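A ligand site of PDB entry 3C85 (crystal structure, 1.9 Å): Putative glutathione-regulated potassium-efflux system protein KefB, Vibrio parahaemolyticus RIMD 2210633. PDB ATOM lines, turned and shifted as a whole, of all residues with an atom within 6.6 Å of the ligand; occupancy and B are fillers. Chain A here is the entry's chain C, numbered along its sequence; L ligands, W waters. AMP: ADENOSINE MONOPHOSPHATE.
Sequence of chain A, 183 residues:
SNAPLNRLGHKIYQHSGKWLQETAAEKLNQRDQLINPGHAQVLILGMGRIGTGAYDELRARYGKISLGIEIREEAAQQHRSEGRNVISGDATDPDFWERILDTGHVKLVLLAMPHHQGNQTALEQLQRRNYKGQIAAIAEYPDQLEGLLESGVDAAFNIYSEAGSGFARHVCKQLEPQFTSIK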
ATOM      1  N   LEU A  45     -12.134   0.354 -18.976  1.00  0.00           N
ATOM      2  CA  LEU A  45     -12.511  -0.741 -18.062  1.00  0.00           C
ATOM      3  C   LEU A  45     -12.923  -0.167 -16.709  1.00  0.00           C
ATOM      4  O   LEU A  45     -12.062   0.338 -15.976  1.00  0.00           O
ATOM      5  CB  LEU A  45     -11.356  -1.748 -17.952  1.00  0.00           C
ATOM      6  CG  LEU A  45     -10.792  -2.322 -19.245  1.00  0.00           C
ATOM      7  CD1 LEU A  45      -9.579  -3.279 -19.033  1.00  0.00           C
ATOM      8  CD2 LEU A  45     -11.911  -3.073 -20.092  1.00  0.00           C
ATOM      9  N   GLY A  46     -14.232  -0.259 -16.412  1.00  0.00           N
ATOM     10  CA  GLY A  46     -14.900   0.377 -15.264  1.00  0.00           C
ATOM     11  C   GLY A  46     -15.600   1.616 -15.781  1.00  0.00           C
ATOM     12  O   GLY A  46     -14.968   2.479 -16.401  1.00  0.00           O
ATOM     13  N   MET A  47     -16.919   1.654 -15.586  1.00  0.00           N
ATOM     14  CA  MET A  47     -17.721   2.807 -15.982  1.00  0.00           C
ATOM     15  C   MET A  47     -18.452   3.394 -14.776  1.00  0.00           C
ATOM     16  O   MET A  47     -19.631   3.770 -14.877  1.00  0.00           O
ATOM     17  CB  MET A  47     -18.654   2.434 -17.123  1.00  0.00           C
ATOM     18  CG  MET A  47     -17.911   2.257 -18.469  1.00  0.00           C
ATOM     19  SD  MET A  47     -17.122   3.893 -19.188  1.00  0.00           S
ATOM     20  CE  MET A  47     -18.747   4.952 -19.512  1.00  0.00           C
ATOM     21  N   GLY A  48     -17.746   3.476 -13.648  1.00  0.00           N
ATOM     22  CA  GLY A  48     -18.199   4.344 -12.550  1.00  0.00           C
ATOM     23  C   GLY A  48     -17.971   5.789 -12.920  1.00  0.00           C
ATOM     24  O   GLY A  48     -17.801   6.135 -14.118  1.00  0.00           O
ATOM     25  N   ARG A  49     -17.972   6.681 -11.942  1.00  0.00           N
ATOM     26  CA  ARG A  49     -17.833   8.115 -12.303  1.00  0.00           C
ATOM     27  C   ARG A  49     -16.523   8.439 -13.017  1.00  0.00           C
ATOM     28  O   ARG A  49     -16.475   9.269 -13.921  1.00  0.00           O
ATOM     29  CB  ARG A  49     -18.113   9.058 -11.108  1.00  0.00           C
ATOM     30  CG  ARG A  49     -19.565   8.897 -10.641  1.00  0.00           C
ATOM     31  CD  ARG A  49     -20.001   9.935  -9.600  1.00  0.00           C
ATOM     32  NE  ARG A  49     -21.464   9.882  -9.476  1.00  0.00           N
ATOM     33  CZ  ARG A  49     -22.126   9.148  -8.586  1.00  0.00           C
ATOM     34  NH1 ARG A  49     -21.473   8.416  -7.674  1.00  0.00           N
ATOM     35  NH2 ARG A  49     -23.454   9.152  -8.615  1.00  0.00           N
ATOM     36  N   ILE A  50     -15.449   7.733 -12.648  1.00  0.00           N
ATOM     37  CA  ILE A  50     -14.178   7.923 -13.302  1.00  0.00           C
ATOM     38  C   ILE A  50     -14.190   7.548 -14.753  1.00  0.00           C
ATOM     39  O   ILE A  50     -13.857   8.411 -15.589  1.00  0.00           O
ATOM     40  CB  ILE A  50     -13.027   7.197 -12.581  1.00  0.00           C
ATOM     41  CG1 ILE A  50     -12.955   7.668 -11.118  1.00  0.00           C
ATOM     42  CG2 ILE A  50     -11.687   7.425 -13.351  1.00  0.00           C
ATOM     43  CD1 ILE A  50     -11.896   6.902 -10.282  1.00  0.00           C
ATOM     44  N   GLY A  51     -14.537   6.274 -15.042  1.00  0.00           N
ATOM     45  CA  GLY A  51     -14.626   5.743 -16.409  1.00  0.00           C
ATOM     46  C   GLY A  51     -15.514   6.603 -17.269  1.00  0.00           C
ATOM     47  O   GLY A  51     -15.197   6.903 -18.424  1.00  0.00           O
ATOM     48  N   ILE A  69     -16.659  -0.859 -20.381  1.00  0.00           N
ATOM     49  CA  ILE A  69     -16.998  -2.171 -19.823  1.00  0.00           C
ATOM     50  C   ILE A  69     -17.349  -2.022 -18.358  1.00  0.00           C
ATOM     51  O   ILE A  69     -16.592  -1.399 -17.623  1.00  0.00           O
ATOM     52  CB  ILE A  69     -15.822  -3.209 -19.990  1.00  0.00           C
ATOM     53  CG1 ILE A  69     -15.354  -3.298 -21.447  1.00  0.00           C
ATOM     54  CG2 ILE A  69     -16.230  -4.605 -19.428  1.00  0.00           C
ATOM     55  CD1 ILE A  69     -16.417  -3.744 -22.483  1.00  0.00           C
ATOM     56  N   GLU A  70     -18.495  -2.571 -17.963  1.00  0.00           N
ATOM     57  CA  GLU A  70     -19.052  -2.360 -16.652  1.00  0.00           C
ATOM     58  C   GLU A  70     -19.638  -3.669 -16.161  1.00  0.00           C
ATOM     59  O   GLU A  70     -20.494  -4.245 -16.824  1.00  0.00           O
ATOM     60  CB  GLU A  70     -20.135  -1.254 -16.707  1.00  0.00           C
ATOM     61  CG  GLU A  70     -20.896  -1.018 -15.381  1.00  0.00           C
ATOM     62  CD  GLU A  70     -19.996  -0.845 -14.195  1.00  0.00           C
ATOM     63  OE1 GLU A  70     -19.085   0.029 -14.265  1.00  0.00           O
ATOM     64  OE2 GLU A  70     -20.206  -1.570 -13.185  1.00  0.00           O
ATOM     65  N   ILE A  71     -19.165  -4.142 -15.014  1.00  0.00           N
ATOM     66  CA  ILE A  71     -19.609  -5.431 -14.466  1.00  0.00           C
ATOM     67  C   ILE A  71     -21.076  -5.408 -13.985  1.00  0.00           C
ATOM     68  O   ILE A  71     -21.779  -6.396 -14.120  1.00  0.00           O
ATOM     69  CB  ILE A  71     -18.657  -5.934 -13.352  1.00  0.00           C
ATOM     70  CG1 ILE A  71     -18.839  -7.445 -13.092  1.00  0.00           C
ATOM     71  CG2 ILE A  71     -18.746  -5.084 -12.078  1.00  0.00           C
ATOM     72  CD1 ILE A  71     -17.633  -8.074 -12.401  1.00  0.00           C
ATOM     73  N   ARG A  72     -21.518  -4.257 -13.456  1.00  0.00           N
ATOM     74  CA  ARG A  72     -22.872  -4.091 -12.895  1.00  0.00           C
ATOM     75  C   ARG A  72     -23.848  -3.935 -14.058  1.00  0.00           C
ATOM     76  O   ARG A  72     -23.825  -2.926 -14.749  1.00  0.00           O
ATOM     77  CB  ARG A  72     -22.919  -2.855 -11.984  1.00  0.00           C
ATOM     78  CG  ARG A  72     -22.214  -3.050 -10.616  1.00  0.00           C
ATOM     79  CD  ARG A  72     -22.319  -1.821  -9.684  1.00  0.00           C
ATOM     80  NE  ARG A  72     -21.516  -0.694 -10.150  1.00  0.00           N
ATOM     81  CZ  ARG A  72     -21.984   0.529 -10.359  1.00  0.00           C
ATOM     82  NH1 ARG A  72     -23.268   0.793 -10.105  1.00  0.00           N
ATOM     83  NH2 ARG A  72     -21.183   1.506 -10.794  1.00  0.00           N
ATOM     84  N   ALA A  75     -26.069  -0.663 -14.127  1.00  0.00           N
ATOM     85  CA  ALA A  75     -25.208   0.458 -14.512  1.00  0.00           C
ATOM     86  C   ALA A  75     -24.925   0.482 -16.019  1.00  0.00           C
ATOM     87  O   ALA A  75     -24.879   1.545 -16.617  1.00  0.00           O
ATOM     88  CB  ALA A  75     -23.862   0.413 -13.743  1.00  0.00           C
ATOM     89  N   HIS A  79     -26.150   3.370 -18.684  1.00  0.00           N
ATOM     90  CA  HIS A  79     -25.241   4.037 -19.636  1.00  0.00           C
ATOM     91  C   HIS A  79     -25.768   3.980 -21.056  1.00  0.00           C
ATOM     92  O   HIS A  79     -25.697   4.965 -21.800  1.00  0.00           O
ATOM     93  CB  HIS A  79     -23.830   3.410 -19.566  1.00  0.00           C
ATOM     94  CG  HIS A  79     -22.991   3.955 -18.446  1.00  0.00           C
ATOM     95  ND1 HIS A  79     -22.752   5.297 -18.291  1.00  0.00           N
ATOM     96  CD2 HIS A  79     -22.353   3.337 -17.430  1.00  0.00           C
ATOM     97  CE1 HIS A  79     -22.005   5.488 -17.220  1.00  0.00           C
ATOM     98  NE2 HIS A  79     -21.754   4.310 -16.671  1.00  0.00           N
ATOM     99  N   GLY A  89     -19.840  -6.873 -18.472  1.00  0.00           N
ATOM    100  CA  GLY A  89     -18.907  -7.961 -18.556  1.00  0.00           C
ATOM    101  C   GLY A  89     -17.860  -7.758 -17.499  1.00  0.00           C
ATOM    102  O   GLY A  89     -17.792  -6.715 -16.872  1.00  0.00           O
ATOM    103  N   ASP A  90     -17.041  -8.777 -17.300  1.00  0.00           N
ATOM    104  CA  ASP A  90     -16.082  -8.824 -16.257  1.00  0.00           C
ATOM    105  C   ASP A  90     -14.657  -8.764 -16.834  1.00  0.00           C
ATOM    106  O   ASP A  90     -14.175  -9.739 -17.430  1.00  0.00           O
ATOM    107  CB  ASP A  90     -16.296 -10.138 -15.480  1.00  0.00           C
ATOM    108  CG  ASP A  90     -15.331 -10.312 -14.323  1.00  0.00           C
ATOM    109  OD1 ASP A  90     -14.412  -9.495 -14.127  1.00  0.00           O
ATOM    110  OD2 ASP A  90     -15.490 -11.318 -13.606  1.00  0.00           O
ATOM    111  N   ALA A  91     -13.999  -7.618 -16.632  1.00  0.00           N
ATOM    112  CA  ALA A  91     -12.666  -7.366 -17.180  1.00  0.00           C
ATOM    113  C   ALA A  91     -11.581  -8.211 -16.490  1.00  0.00           C
ATOM    114  O   ALA A  91     -10.417  -8.162 -16.883  1.00  0.00           O
ATOM    115  CB  ALA A  91     -12.348  -5.889 -17.052  1.00  0.00           C
ATOM    116  N   THR A  92     -11.931  -8.979 -15.470  1.00  0.00           N
ATOM    117  CA  THR A  92     -10.934  -9.894 -14.909  1.00  0.00           C
ATOM    118  C   THR A  92     -11.062 -11.319 -15.417  1.00  0.00           C
ATOM    119  O   THR A  92     -10.288 -12.182 -15.012  1.00  0.00           O
ATOM    120  CB  THR A  92     -10.946  -9.893 -13.368  1.00  0.00           C
ATOM    121  OG1 THR A  92     -12.121 -10.577 -12.893  1.00  0.00           O
ATOM    122  CG2 THR A  92     -10.910  -8.447 -12.872  1.00  0.00           C
ATOM    123  N   ASP A  93     -12.028 -11.573 -16.301  1.00  0.00           N
ATOM    124  CA  ASP A  93     -12.360 -12.921 -16.766  1.00  0.00           C
ATOM    125  C   ASP A  93     -11.650 -13.187 -18.100  1.00  0.00           C
ATOM    126  O   ASP A  93     -11.930 -12.505 -19.103  1.00  0.00           O
ATOM    127  CB  ASP A  93     -13.890 -13.074 -16.857  1.00  0.00           C
ATOM    128  CG  ASP A  93     -14.334 -14.412 -17.442  1.00  0.00           C
ATOM    129  OD1 ASP A  93     -13.567 -15.390 -17.407  1.00  0.00           O
ATOM    130  OD2 ASP A  93     -15.477 -14.458 -17.950  1.00  0.00           O
ATOM    131  N   ALA A 112      -9.862   1.910 -15.064  1.00  0.00           N
ATOM    132  CA  ALA A 112     -10.566   2.846 -14.212  1.00  0.00           C
ATOM    133  C   ALA A 112     -11.313   2.044 -13.152  1.00  0.00           C
ATOM    134  O   ALA A 112     -12.505   2.280 -12.868  1.00  0.00           O
ATOM    135  CB  ALA A 112     -11.554   3.725 -15.030  1.00  0.00           C
ATOM    136  N   MET A 113     -10.574   1.102 -12.563  1.00  0.00           N
ATOM    137  CA  MET A 113     -11.081   0.274 -11.455  1.00  0.00           C
ATOM    138  C   MET A 113     -10.116   0.374 -10.263  1.00  0.00           C
ATOM    139  O   MET A 113      -9.417  -0.621  -9.936  1.00  0.00           O
ATOM    140  CB  MET A 113     -11.299  -1.192 -11.910  1.00  0.00           C
ATOM    141  CG  MET A 113     -12.312  -1.363 -13.062  1.00  0.00           C
ATOM    142  SD  MET A 113     -12.055  -3.023 -14.046  1.00  0.00           S
ATOM    143  CE  MET A 113     -10.298  -2.625 -14.754  1.00  0.00           C
ATOM    144  N   PRO A 114     -10.091   1.550  -9.566  1.00  0.00           N
ATOM    145  CA  PRO A 114      -9.064   1.775  -8.534  1.00  0.00           C
ATOM    146  C   PRO A 114      -9.336   1.077  -7.204  1.00  0.00           C
ATOM    147  O   PRO A 114      -8.517   1.170  -6.278  1.00  0.00           O
ATOM    148  CB  PRO A 114      -9.053   3.325  -8.361  1.00  0.00           C
ATOM    149  CG  PRO A 114     -10.465   3.775  -8.760  1.00  0.00           C
ATOM    150  CD  PRO A 114     -11.006   2.707  -9.735  1.00  0.00           C
ATOM    151  N   HIS A 115     -10.426   0.356  -7.085  1.00  0.00           N
ATOM    152  CA  HIS A 115     -10.644  -0.436  -5.876  1.00  0.00           C
ATOM    153  C   HIS A 115     -10.583  -1.935  -6.096  1.00  0.00           C
ATOM    154  O   HIS A 115     -10.718  -2.411  -7.187  1.00  0.00           O
ATOM    155  CB  HIS A 115     -11.907  -0.018  -5.132  1.00  0.00           C
ATOM    156  CG  HIS A 115     -12.015   1.443  -4.860  1.00  0.00           C
ATOM    157  ND1 HIS A 115     -12.554   2.317  -5.756  1.00  0.00           N
ATOM    158  CD2 HIS A 115     -11.641   2.184  -3.797  1.00  0.00           C
ATOM    159  CE1 HIS A 115     -12.490   3.538  -5.278  1.00  0.00           C
ATOM    160  NE2 HIS A 115     -11.953   3.487  -4.087  1.00  0.00           N
ATOM    161  N   HIS A 116     -10.357  -2.665  -5.024  1.00  0.00           N
ATOM    162  CA  HIS A 116     -10.320  -4.098  -5.060  1.00  0.00           C
ATOM    163  C   HIS A 116      -9.366  -4.739  -6.036  1.00  0.00           C
ATOM    164  O   HIS A 116      -9.669  -5.773  -6.558  1.00  0.00           O
ATOM    165  CB  HIS A 116     -11.708  -4.670  -5.252  1.00  0.00           C
ATOM    166  CG  HIS A 116     -12.720  -4.102  -4.311  1.00  0.00           C
ATOM    167  ND1 HIS A 116     -13.687  -3.226  -4.717  1.00  0.00           N
ATOM    168  CD2 HIS A 116     -12.884  -4.256  -2.981  1.00  0.00           C
ATOM    169  CE1 HIS A 116     -14.413  -2.857  -3.685  1.00  0.00           C
ATOM    170  NE2 HIS A 116     -13.942  -3.468  -2.609  1.00  0.00           N
ATOM    171  N   GLY A 118      -8.836  -4.198  -8.937  1.00  0.00           N
ATOM    172  CA  GLY A 118      -9.421  -4.316 -10.293  1.00  0.00           C
ATOM    173  C   GLY A 118      -8.427  -3.956 -11.378  1.00  0.00           C
ATOM    174  O   GLY A 118      -8.245  -4.708 -12.321  1.00  0.00           O
ATOM    175  N   ASN A 119      -7.772  -2.821 -11.254  1.00  0.00           N
ATOM    176  CA  ASN A 119      -6.805  -2.403 -12.243  1.00  0.00           C
ATOM    177  C   ASN A 119      -5.708  -3.455 -12.509  1.00  0.00           C
ATOM    178  O   ASN A 119      -5.395  -3.762 -13.647  1.00  0.00           O
ATOM    179  CB  ASN A 119      -6.153  -1.079 -11.796  1.00  0.00           C
ATOM    180  CG  ASN A 119      -7.030   0.157 -12.107  1.00  0.00           C
ATOM    181  OD1 ASN A 119      -8.026   0.089 -12.840  1.00  0.00           O
ATOM    182  ND2 ASN A 119      -6.629   1.310 -11.534  1.00  0.00           N
ATOM    183  N   ALA A 122      -7.181  -6.792 -14.083  1.00  0.00           N
ATOM    184  CA  ALA A 122      -7.467  -6.617 -15.511  1.00  0.00           C
ATOM    185  C   ALA A 122      -6.194  -6.501 -16.330  1.00  0.00           C
ATOM    186  O   ALA A 122      -6.122  -7.041 -17.460  1.00  0.00           O
ATOM    187  CB  ALA A 122      -8.338  -5.395 -15.742  1.00  0.00           C
HETATM  188  P   AMP L   1     -14.312   0.374  -8.183  1.00  0.00           P
HETATM  189  O1P AMP L   1     -14.398   1.832  -7.764  1.00  0.00           O
HETATM  190  O2P AMP L   1     -12.946  -0.125  -8.597  1.00  0.00           O
HETATM  191  O3P AMP L   1     -15.118  -0.474  -7.234  1.00  0.00           O
HETATM  192  O5' AMP L   1     -15.124   0.337  -9.579  1.00  0.00           O
HETATM  193  C5' AMP L   1     -15.379   1.510 -10.353  1.00  0.00           C
HETATM  194  C4' AMP L   1     -16.330   1.079 -11.471  1.00  0.00           C
HETATM  195  O4' AMP L   1     -15.769  -0.081 -12.103  1.00  0.00           O
HETATM  196  C3' AMP L   1     -17.699   0.672 -10.935  1.00  0.00           C
HETATM  197  O3' AMP L   1     -18.739   1.097 -11.830  1.00  0.00           O
HETATM  198  C2' AMP L   1     -17.636  -0.849 -10.961  1.00  0.00           C
HETATM  199  O2' AMP L   1     -18.898  -1.550 -10.989  1.00  0.00           O
HETATM  200  C1' AMP L   1     -16.766  -1.105 -12.179  1.00  0.00           C
HETATM  201  N9  AMP L   1     -16.083  -2.430 -12.129  1.00  0.00           N
HETATM  202  C8  AMP L   1     -15.509  -2.985 -11.024  1.00  0.00           C
HETATM  203  N7  AMP L   1     -14.951  -4.182 -11.329  1.00  0.00           N
HETATM  204  C5  AMP L   1     -15.151  -4.411 -12.660  1.00  0.00           C
HETATM  205  C6  AMP L   1     -14.822  -5.520 -13.596  1.00  0.00           C
HETATM  206  N6  AMP L   1     -14.144  -6.592 -13.094  1.00  0.00           N
HETATM  207  N1  AMP L   1     -15.220  -5.406 -14.916  1.00  0.00           N
HETATM  208  C2  AMP L   1     -15.871  -4.294 -15.309  1.00  0.00           C
HETATM  209  N3  AMP L   1     -16.223  -3.270 -14.488  1.00  0.00           N
HETATM  210  C4  AMP L   1     -15.907  -3.259 -13.174  1.00  0.00           C
HETATM  211  O   HOH W   1     -18.607  -3.397  -9.119  1.00  0.00           O
HETATM  212  O   HOH W   2     -15.231   4.803  -9.506  1.00  0.00           O
HETATM  213  O   HOH W   3     -12.448  -3.102  -9.113  1.00  0.00           O
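The guanidinium group (NE) of Arg 72 lies within salt-bridge range of the side-chain carboxylate (OE2) of Glu 70 (3.4 Å). The side-chain carboxylate (OE1) of Glu 70 is in hydrogen-bond range of the backbone NH (N) of Met 47 (3.0 Å). OD1 of Asp 90 sits at hydrogen-bond distance from OG1 of Thr 92 (2.8 Å). N of Ile 71 lies close to O of Gly 89 (3.5 Å). The backbone carbonyl oxygen (O) of Ile 69 sits at hydrogen-bond distance from the backbone NH (N) of Gly 46 (2.9 Å). N of Met 113 is in hydrogen-bond range of OD1 of Asn 119. The backbone NH (N) of Ala 112 is in hydrogen-bond range of the backbone carbonyl oxygen (O) of Leu 45 (2.9 Å). N of Ala 112 sits at hydrogen-bond distance from OD1 of Asn 119.
Water W3 bridges O of His 115 (2.7 Å) and O2P of the ligand (3.1 Å).
O of Gly 89 lies close to N1 of the ligand. An oxygen (O2P) of the ligand sits close to the backbone nitrogen (N) of Pro 114 (3.4 Å). Gly 46 touches the ligand (CA to O4', 3.3 Å). C of Met 47 touches O3' of the ligand, 3.7 Å away. Ile 69 touches the ligand (O to N3, 3.7 Å). Thr 92 touches the ligand. Ala 112 touches the ligand. C of Met 113 touches O2P of the ligand, 3.3 Å away. ND1 of His 116 touches O3P of the ligand, 3.99 Å away.
OE2 of Glu 70 lies within hydrogen-bond range of O2' of the ligand (2.6 Å). The guanidinium group (NH2) of Arg 72 is in hydrogen-bond range of an oxygen (O3') of the ligand, at 2.7 Å. The backbone NH (N) of His 115 lies within hydrogen-bond range of an oxygen (O2P) of the ligand (3.0 Å). A ring nitrogen (ND1) of His 115 is in hydrogen-bond range of an oxygen (O1P) of the ligand, 2.8 Å away. The backbone NH of Ala 91 lies within hydrogen-bond range of a nitrogen (N1) of the ligand (3.1 Å). A nitrogen (N6) of the ligand is in hydrogen-bond range of the side-chain carboxylate of Asp 90, 3.1 Å away. N3 of the ligand sits at hydrogen-bond distance from N of Ile 71 (3.1 Å). An oxygen (O3') of the ligand lies within hydrogen-bond range of the backbone NH (N) of Gly 48 (3.2 Å).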
